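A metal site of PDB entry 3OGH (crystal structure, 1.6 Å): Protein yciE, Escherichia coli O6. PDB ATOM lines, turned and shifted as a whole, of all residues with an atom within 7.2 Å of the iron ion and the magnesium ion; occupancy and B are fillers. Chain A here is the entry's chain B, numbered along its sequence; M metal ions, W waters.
The iron ion is bound by OE1 of Glu 110 (2.0 Å), OE1 of Glu 107 (2.0 Å), OE1 of Glu 140 (2.1 Å), water W2 (2.1 Å), NE2 of His 48 (2.2 Å) and water W1 (2.5 Å). The iron ion has six donor atoms within binding distance. Slightly farther from the iron ion lies the side-chain carboxylate (OE2) of Glu 107 (2.8 Å).
The nearest printed residue that does not touch the iron ion is Thr 52 (4.4 Å).
The magnesium ion is bound by the side-chain carboxylate (OE2) of Glu 110 (1.9 Å), the side-chain amide oxygen (OE1) of Gln 55 (2.0 Å), the side-chain carboxylate (OE2) of Glu 140 (2.0 Å), the side-chain carboxylate (OE2) of Glu 21 (2.0 Å), the side-chain carboxylate (OE1) of Glu 21 (2.1 Å) and water W2 (2.1 Å). The magnesium ion has six donor atoms within binding distance.
OE2 of Glu 139 lies within hydrogen-bond range of NE2 of Gln 55 (2.9 Å). OE1 of Glu 21 lies close to OH of Tyr 114 (2.7 Å). The side-chain hydroxyl (OG1) of Thr 52 is in hydrogen-bond range of the backbone carbonyl oxygen (O) of His 48 (2.8 Å). ND1 of His 48 lies within hydrogen-bond range of OE1 of Glu 51 (2.8 Å).
Four residues have an atom within 4 Å of the magnesium ion: Glu 21, Gln 55, Glu 110 and Glu 140.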
ATOM      1  N   ALA A  17      -8.991  -7.972  30.530  1.00  0.00           N
ATOM      2  CA  ALA A  17      -9.616  -7.334  29.383  1.00  0.00           C
ATOM      3  C   ALA A  17      -9.542  -5.816  29.496  1.00  0.00           C
ATOM      4  O   ALA A  17      -9.243  -5.148  28.492  1.00  0.00           O
ATOM      5  CB  ALA A  17     -11.067  -7.816  29.200  1.00  0.00           C
ATOM      6  N   MET A  20      -6.023  -4.886  28.587  1.00  0.00           N
ATOM      7  CA  MET A  20      -5.900  -5.060  27.143  1.00  0.00           C
ATOM      8  C   MET A  20      -6.471  -3.890  26.395  1.00  0.00           C
ATOM      9  O   MET A  20      -5.850  -3.518  25.379  1.00  0.00           O
ATOM     10  CB  MET A  20      -6.629  -6.355  26.733  1.00  0.00           C
ATOM     11  CG  MET A  20      -6.663  -6.640  25.296  1.00  0.00           C
ATOM     12  SD  MET A  20      -7.692  -8.258  24.957  1.00  0.00           S
ATOM     13  CE  MET A  20      -9.350  -7.446  25.085  1.00  0.00           C
ATOM     14  N   GLU A  21      -7.595  -3.306  26.814  1.00  0.00           N
ATOM     15  CA  GLU A  21      -8.133  -2.170  26.150  1.00  0.00           C
ATOM     16  C   GLU A  21      -7.282  -0.926  26.389  1.00  0.00           C
ATOM     17  O   GLU A  21      -7.155  -0.096  25.499  1.00  0.00           O
ATOM     18  CB  GLU A  21      -9.531  -1.869  26.548  1.00  0.00           C
ATOM     19  CG  GLU A  21     -10.507  -3.025  26.066  1.00  0.00           C
ATOM     20  CD  GLU A  21     -10.579  -3.218  24.612  1.00  0.00           C
ATOM     21  OE1 GLU A  21     -11.345  -4.118  24.127  1.00  0.00           O
ATOM     22  OE2 GLU A  21     -10.079  -2.425  23.797  1.00  0.00           O
ATOM     23  N   ALA A  24      -4.675  -1.401  23.875  1.00  0.00           N
ATOM     24  CA  ALA A  24      -5.204  -1.066  22.544  1.00  0.00           C
ATOM     25  C   ALA A  24      -5.278   0.406  22.285  1.00  0.00           C
ATOM     26  O   ALA A  24      -4.909   0.895  21.168  1.00  0.00           O
ATOM     27  CB  ALA A  24      -6.661  -1.675  22.355  1.00  0.00           C
ATOM     28  N   GLU A  25      -5.726   1.166  23.284  1.00  0.00           N
ATOM     29  CA  GLU A  25      -5.950   2.570  23.154  1.00  0.00           C
ATOM     30  C   GLU A  25      -4.581   3.274  22.874  1.00  0.00           C
ATOM     31  O   GLU A  25      -4.486   4.073  21.979  1.00  0.00           O
ATOM     32  CB  GLU A  25      -6.632   3.105  24.424  1.00  0.00           C
ATOM     33  CG  GLU A  25      -6.680   4.596  24.513  1.00  0.00           C
ATOM     34  CD  GLU A  25      -7.220   5.037  25.913  1.00  0.00           C
ATOM     35  OE1 GLU A  25      -6.788   4.514  26.996  1.00  0.00           O
ATOM     36  OE2 GLU A  25      -8.059   5.919  25.923  1.00  0.00           O
ATOM     37  N   LEU A  28      -3.335   2.187  19.249  1.00  0.00           N
ATOM     38  CA  LEU A  28      -4.080   2.796  18.153  1.00  0.00           C
ATOM     39  C   LEU A  28      -3.668   4.248  17.996  1.00  0.00           C
ATOM     40  O   LEU A  28      -3.454   4.748  16.862  1.00  0.00           O
ATOM     41  CB  LEU A  28      -5.581   2.741  18.356  1.00  0.00           C
ATOM     42  CG  LEU A  28      -6.113   1.303  18.241  1.00  0.00           C
ATOM     43  CD1 LEU A  28      -7.496   1.113  18.967  1.00  0.00           C
ATOM     44  CD2 LEU A  28      -6.175   0.758  16.836  1.00  0.00           C
ATOM     45  N   HIS A  48     -11.424   3.451  15.189  1.00  0.00           N
ATOM     46  CA  HIS A  48     -11.385   2.358  16.166  1.00  0.00           C
ATOM     47  C   HIS A  48     -10.872   2.837  17.494  1.00  0.00           C
ATOM     48  O   HIS A  48     -11.207   2.294  18.542  1.00  0.00           O
ATOM     49  CB  HIS A  48     -10.565   1.158  15.643  1.00  0.00           C
ATOM     50  CG  HIS A  48     -10.815  -0.103  16.417  1.00  0.00           C
ATOM     51  ND1 HIS A  48     -12.096  -0.622  16.538  1.00  0.00           N
ATOM     52  CD2 HIS A  48      -9.997  -0.916  17.131  1.00  0.00           C
ATOM     53  CE1 HIS A  48     -12.028  -1.726  17.276  1.00  0.00           C
ATOM     54  NE2 HIS A  48     -10.755  -1.948  17.635  1.00  0.00           N
ATOM     55  N   GLU A  51     -13.810   4.023  19.148  1.00  0.00           N
ATOM     56  CA  GLU A  51     -14.582   2.815  19.570  1.00  0.00           C
ATOM     57  C   GLU A  51     -13.978   2.211  20.826  1.00  0.00           C
ATOM     58  O   GLU A  51     -14.683   1.872  21.808  1.00  0.00           O
ATOM     59  CB  GLU A  51     -14.666   1.761  18.445  1.00  0.00           C
ATOM     60  CG  GLU A  51     -15.411   2.280  17.245  1.00  0.00           C
ATOM     61  CD  GLU A  51     -15.203   1.538  15.862  1.00  0.00           C
ATOM     62  OE1 GLU A  51     -14.182   0.864  15.530  1.00  0.00           O
ATOM     63  OE2 GLU A  51     -16.099   1.793  15.013  1.00  0.00           O
ATOM     64  N   THR A  52     -12.665   2.124  20.889  1.00  0.00           N
ATOM     65  CA  THR A  52     -11.964   1.525  21.995  1.00  0.00           C
ATOM     66  C   THR A  52     -12.086   2.313  23.281  1.00  0.00           C
ATOM     67  O   THR A  52     -12.202   1.739  24.372  1.00  0.00           O
ATOM     68  CB  THR A  52     -10.493   1.391  21.571  1.00  0.00           C
ATOM     69  OG1 THR A  52     -10.418   0.470  20.492  1.00  0.00           O
ATOM     70  CG2 THR A  52      -9.546   0.851  22.716  1.00  0.00           C
ATOM     71  N   GLN A  55     -15.212   1.180  24.565  1.00  0.00           N
ATOM     72  CA  GLN A  55     -15.120  -0.223  25.078  1.00  0.00           C
ATOM     73  C   GLN A  55     -14.608  -0.205  26.537  1.00  0.00           C
ATOM     74  O   GLN A  55     -14.984  -1.018  27.379  1.00  0.00           O
ATOM     75  CB  GLN A  55     -14.176  -1.017  24.238  1.00  0.00           C
ATOM     76  CG  GLN A  55     -14.665  -1.213  22.820  1.00  0.00           C
ATOM     77  CD  GLN A  55     -13.602  -1.908  21.940  1.00  0.00           C
ATOM     78  OE1 GLN A  55     -12.451  -2.263  22.337  1.00  0.00           O
ATOM     79  NE2 GLN A  55     -14.041  -2.293  20.712  1.00  0.00           N
ATOM     80  N   ILE A  56     -13.680   0.698  26.824  1.00  0.00           N
ATOM     81  CA  ILE A  56     -13.172   0.864  28.187  1.00  0.00           C
ATOM     82  C   ILE A  56     -14.299   1.252  29.117  1.00  0.00           C
ATOM     83  O   ILE A  56     -14.385   0.639  30.225  1.00  0.00           O
ATOM     84  CB  ILE A  56     -12.019   1.841  28.242  1.00  0.00           C
ATOM     85  CG1 ILE A  56     -10.766   1.260  27.517  1.00  0.00           C
ATOM     86  CG2 ILE A  56     -11.659   2.160  29.693  1.00  0.00           C
ATOM     87  CD1 ILE A  56      -9.720   2.304  27.154  1.00  0.00           C
ATOM     88  N   LEU A  59     -16.483  -1.798  29.688  1.00  0.00           N
ATOM     89  CA  LEU A  59     -15.880  -2.744  30.620  1.00  0.00           C
ATOM     90  C   LEU A  59     -15.904  -2.259  32.023  1.00  0.00           C
ATOM     91  O   LEU A  59     -16.087  -3.055  32.975  1.00  0.00           O
ATOM     92  CB  LEU A  59     -14.470  -3.070  30.268  1.00  0.00           C
ATOM     93  CG  LEU A  59     -14.225  -3.938  29.105  1.00  0.00           C
ATOM     94  CD1 LEU A  59     -12.702  -4.063  28.814  1.00  0.00           C
ATOM     95  CD2 LEU A  59     -14.771  -5.358  29.315  1.00  0.00           C
ATOM     96  N   GLY A 103      -1.573  -4.794  13.633  1.00  0.00           N
ATOM     97  CA  GLY A 103      -2.880  -4.324  14.075  1.00  0.00           C
ATOM     98  C   GLY A 103      -3.972  -5.365  14.001  1.00  0.00           C
ATOM     99  O   GLY A 103      -4.793  -5.498  14.903  1.00  0.00           O
ATOM    100  N   PHE A 106      -3.528  -7.924  16.794  1.00  0.00           N
ATOM    101  CA  PHE A 106      -4.075  -7.484  18.053  1.00  0.00           C
ATOM    102  C   PHE A 106      -5.575  -7.560  18.103  1.00  0.00           C
ATOM    103  O   PHE A 106      -6.128  -7.979  19.113  1.00  0.00           O
ATOM    104  CB  PHE A 106      -3.624  -6.036  18.419  1.00  0.00           C
ATOM    105  CG  PHE A 106      -3.881  -5.707  19.818  1.00  0.00           C
ATOM    106  CD1 PHE A 106      -2.935  -5.963  20.753  1.00  0.00           C
ATOM    107  CD2 PHE A 106      -5.111  -5.210  20.249  1.00  0.00           C
ATOM    108  CE1 PHE A 106      -3.118  -5.676  22.114  1.00  0.00           C
ATOM    109  CE2 PHE A 106      -5.346  -5.004  21.601  1.00  0.00           C
ATOM    110  CZ  PHE A 106      -4.344  -5.225  22.487  1.00  0.00           C
ATOM    111  N   GLU A 107      -6.273  -7.228  17.018  1.00  0.00           N
ATOM    112  CA  GLU A 107      -7.747  -7.382  17.068  1.00  0.00           C
ATOM    113  C   GLU A 107      -8.134  -8.848  17.245  1.00  0.00           C
ATOM    114  O   GLU A 107      -9.120  -9.109  17.914  1.00  0.00           O
ATOM    115  CB  GLU A 107      -8.461  -6.904  15.733  1.00  0.00           C
ATOM    116  CG  GLU A 107      -8.194  -5.463  15.433  1.00  0.00           C
ATOM    117  CD  GLU A 107      -8.692  -4.561  16.536  1.00  0.00           C
ATOM    118  OE1 GLU A 107      -9.781  -4.717  17.205  1.00  0.00           O
ATOM    119  OE2 GLU A 107      -7.992  -3.604  16.845  1.00  0.00           O
ATOM    120  N   GLN A 108      -7.378  -9.773  16.680  1.00  0.00           N
ATOM    121  CA  GLN A 108      -7.683 -11.182  16.791  1.00  0.00           C
ATOM    122  C   GLN A 108      -7.413 -11.678  18.233  1.00  0.00           C
ATOM    123  O   GLN A 108      -8.038 -12.550  18.734  1.00  0.00           O
ATOM    124  CB  GLN A 108      -6.922 -11.981  15.739  1.00  0.00           C
ATOM    125  CG  GLN A 108      -7.486 -11.745  14.377  1.00  0.00           C
ATOM    126  CD  GLN A 108      -8.868 -12.399  14.225  1.00  0.00           C
ATOM    127  OE1 GLN A 108      -9.364 -13.043  15.123  1.00  0.00           O
ATOM    128  NE2 GLN A 108      -9.519 -12.192  13.023  1.00  0.00           N
ATOM    129  N   GLU A 110      -7.969  -9.725  20.802  1.00  0.00           N
ATOM    130  CA  GLU A 110      -9.161  -9.278  21.458  1.00  0.00           C
ATOM    131  C   GLU A 110     -10.321 -10.215  21.203  1.00  0.00           C
ATOM    132  O   GLU A 110     -11.088 -10.534  22.134  1.00  0.00           O
ATOM    133  CB  GLU A 110      -9.570  -7.855  21.096  1.00  0.00           C
ATOM    134  CG  GLU A 110      -8.404  -6.832  21.376  1.00  0.00           C
ATOM    135  CD  GLU A 110      -8.956  -5.389  21.108  1.00  0.00           C
ATOM    136  OE1 GLU A 110      -9.134  -5.035  19.849  1.00  0.00           O
ATOM    137  OE2 GLU A 110      -9.416  -4.615  22.013  1.00  0.00           O
ATOM    138  N   ILE A 111     -10.477 -10.613  19.957  1.00  0.00           N
ATOM    139  CA  ILE A 111     -11.553 -11.546  19.626  1.00  0.00           C
ATOM    140  C   ILE A 111     -11.494 -12.830  20.432  1.00  0.00           C
ATOM    141  O   ILE A 111     -12.500 -13.319  20.981  1.00  0.00           O
ATOM    142  CB  ILE A 111     -11.538 -11.782  18.098  1.00  0.00           C
ATOM    143  CG1 ILE A 111     -12.062 -10.554  17.366  1.00  0.00           C
ATOM    144  CG2 ILE A 111     -12.514 -13.021  17.694  1.00  0.00           C
ATOM    145  CD1 ILE A 111     -11.700 -10.538  15.865  1.00  0.00           C
ATOM    146  N   TYR A 114     -12.317 -12.116  24.177  1.00  0.00           N
ATOM    147  CA  TYR A 114     -13.729 -11.875  24.441  1.00  0.00           C
ATOM    148  C   TYR A 114     -14.536 -13.142  24.222  1.00  0.00           C
ATOM    149  O   TYR A 114     -15.566 -13.304  24.876  1.00  0.00           O
ATOM    150  CB  TYR A 114     -14.338 -10.711  23.655  1.00  0.00           C
ATOM    151  CG  TYR A 114     -13.846  -9.325  24.213  1.00  0.00           C
ATOM    152  CD1 TYR A 114     -14.044  -9.046  25.526  1.00  0.00           C
ATOM    153  CD2 TYR A 114     -13.132  -8.451  23.421  1.00  0.00           C
ATOM    154  CE1 TYR A 114     -13.645  -7.834  26.049  1.00  0.00           C
ATOM    155  CE2 TYR A 114     -12.691  -7.232  23.959  1.00  0.00           C
ATOM    156  CZ  TYR A 114     -12.912  -6.985  25.255  1.00  0.00           C
ATOM    157  OH  TYR A 114     -12.516  -5.775  25.840  1.00  0.00           O
ATOM    158  N   ILE A 136     -18.946  -5.493  22.346  1.00  0.00           N
ATOM    159  CA  ILE A 136     -17.475  -5.231  22.159  1.00  0.00           C
ATOM    160  C   ILE A 136     -16.850  -6.173  21.135  1.00  0.00           C
ATOM    161  O   ILE A 136     -16.122  -5.774  20.239  1.00  0.00           O
ATOM    162  CB  ILE A 136     -16.710  -5.332  23.529  1.00  0.00           C
ATOM    163  CG1 ILE A 136     -17.267  -4.292  24.465  1.00  0.00           C
ATOM    164  CG2 ILE A 136     -15.226  -5.117  23.274  1.00  0.00           C
ATOM    165  CD1 ILE A 136     -16.720  -4.405  25.887  1.00  0.00           C
ATOM    166  N   GLU A 139     -17.500  -5.336  17.608  1.00  0.00           N
ATOM    167  CA  GLU A 139     -16.696  -4.233  17.091  1.00  0.00           C
ATOM    168  C   GLU A 139     -15.284  -4.688  16.722  1.00  0.00           C
ATOM    169  O   GLU A 139     -14.688  -4.197  15.724  1.00  0.00           O
ATOM    170  CB  GLU A 139     -16.591  -3.071  18.162  1.00  0.00           C
ATOM    171  CG  GLU A 139     -17.737  -2.263  18.284  1.00  0.00           C
ATOM    172  CD  GLU A 139     -17.625  -1.153  19.319  1.00  0.00           C
ATOM    173  OE1 GLU A 139     -18.570  -0.308  19.428  1.00  0.00           O
ATOM    174  OE2 GLU A 139     -16.643  -1.158  20.029  1.00  0.00           O
ATOM    175  N   GLU A 140     -14.697  -5.587  17.519  1.00  0.00           N
ATOM    176  CA  GLU A 140     -13.395  -6.106  17.204  1.00  0.00           C
ATOM    177  C   GLU A 140     -13.408  -6.908  15.901  1.00  0.00           C
ATOM    178  O   GLU A 140     -12.539  -6.793  15.047  1.00  0.00           O
ATOM    179  CB  GLU A 140     -12.840  -6.953  18.372  1.00  0.00           C
ATOM    180  CG  GLU A 140     -12.978  -6.415  19.762  1.00  0.00           C
ATOM    181  CD  GLU A 140     -12.282  -5.091  20.034  1.00  0.00           C
ATOM    182  OE1 GLU A 140     -11.918  -4.304  19.120  1.00  0.00           O
ATOM    183  OE2 GLU A 140     -11.945  -4.857  21.255  1.00  0.00           O
ATOM    184  N   LYS A 141     -14.448  -7.755  15.728  1.00  0.00           N
ATOM    185  CA  LYS A 141     -14.634  -8.539  14.484  1.00  0.00           C
ATOM    186  C   LYS A 141     -14.772  -7.627  13.275  1.00  0.00           C
ATOM    187  O   LYS A 141     -14.160  -7.858  12.247  1.00  0.00           O
ATOM    188  CB  LYS A 141     -15.863  -9.448  14.636  1.00  0.00           C
ATOM    189  CG  LYS A 141     -15.698 -10.637  15.613  1.00  0.00           C
ATOM    190  CD  LYS A 141     -17.043 -11.376  15.760  1.00  0.00           C
ATOM    191  CE  LYS A 141     -16.927 -12.604  16.609  1.00  0.00           C
ATOM    192  NZ  LYS A 141     -18.205 -13.365  16.630  1.00  0.00           N
ATOM    193  N   MET A 143     -13.535  -4.584  12.950  1.00  0.00           N
ATOM    194  CA  MET A 143     -12.214  -4.020  12.695  1.00  0.00           C
ATOM    195  C   MET A 143     -11.312  -5.035  12.099  1.00  0.00           C
ATOM    196  O   MET A 143     -10.620  -4.729  11.090  1.00  0.00           O
ATOM    197  CB  MET A 143     -11.579  -3.495  14.009  1.00  0.00           C
ATOM    198  CG  MET A 143     -10.230  -2.849  13.871  1.00  0.00           C
ATOM    199  SD  MET A 143     -10.280  -1.337  12.666  1.00  0.00           S
ATOM    200  CE  MET A 143      -8.539  -0.607  13.111  1.00  0.00           C
ATOM    201  N   ALA A 144     -11.246  -6.262  12.634  1.00  0.00           N
ATOM    202  CA  ALA A 144     -10.386  -7.290  12.068  1.00  0.00           C
ATOM    203  C   ALA A 144     -10.745  -7.550  10.559  1.00  0.00           C
ATOM    204  O   ALA A 144      -9.882  -7.673   9.708  1.00  0.00           O
ATOM    205  CB  ALA A 144     -10.497  -8.614  12.868  1.00  0.00           C
HETATM  206 FE    FE M   1     -10.003  -3.577  18.823  1.00  0.00          FE
HETATM  207 MG    MG M   2     -10.882  -3.425  22.198  1.00  0.00          MG
HETATM  208  O   HOH W   1      -7.708  -2.517  18.911  1.00  0.00           O
HETATM  209  O   HOH W   2     -10.040  -2.332  20.575  1.00  0.00           O
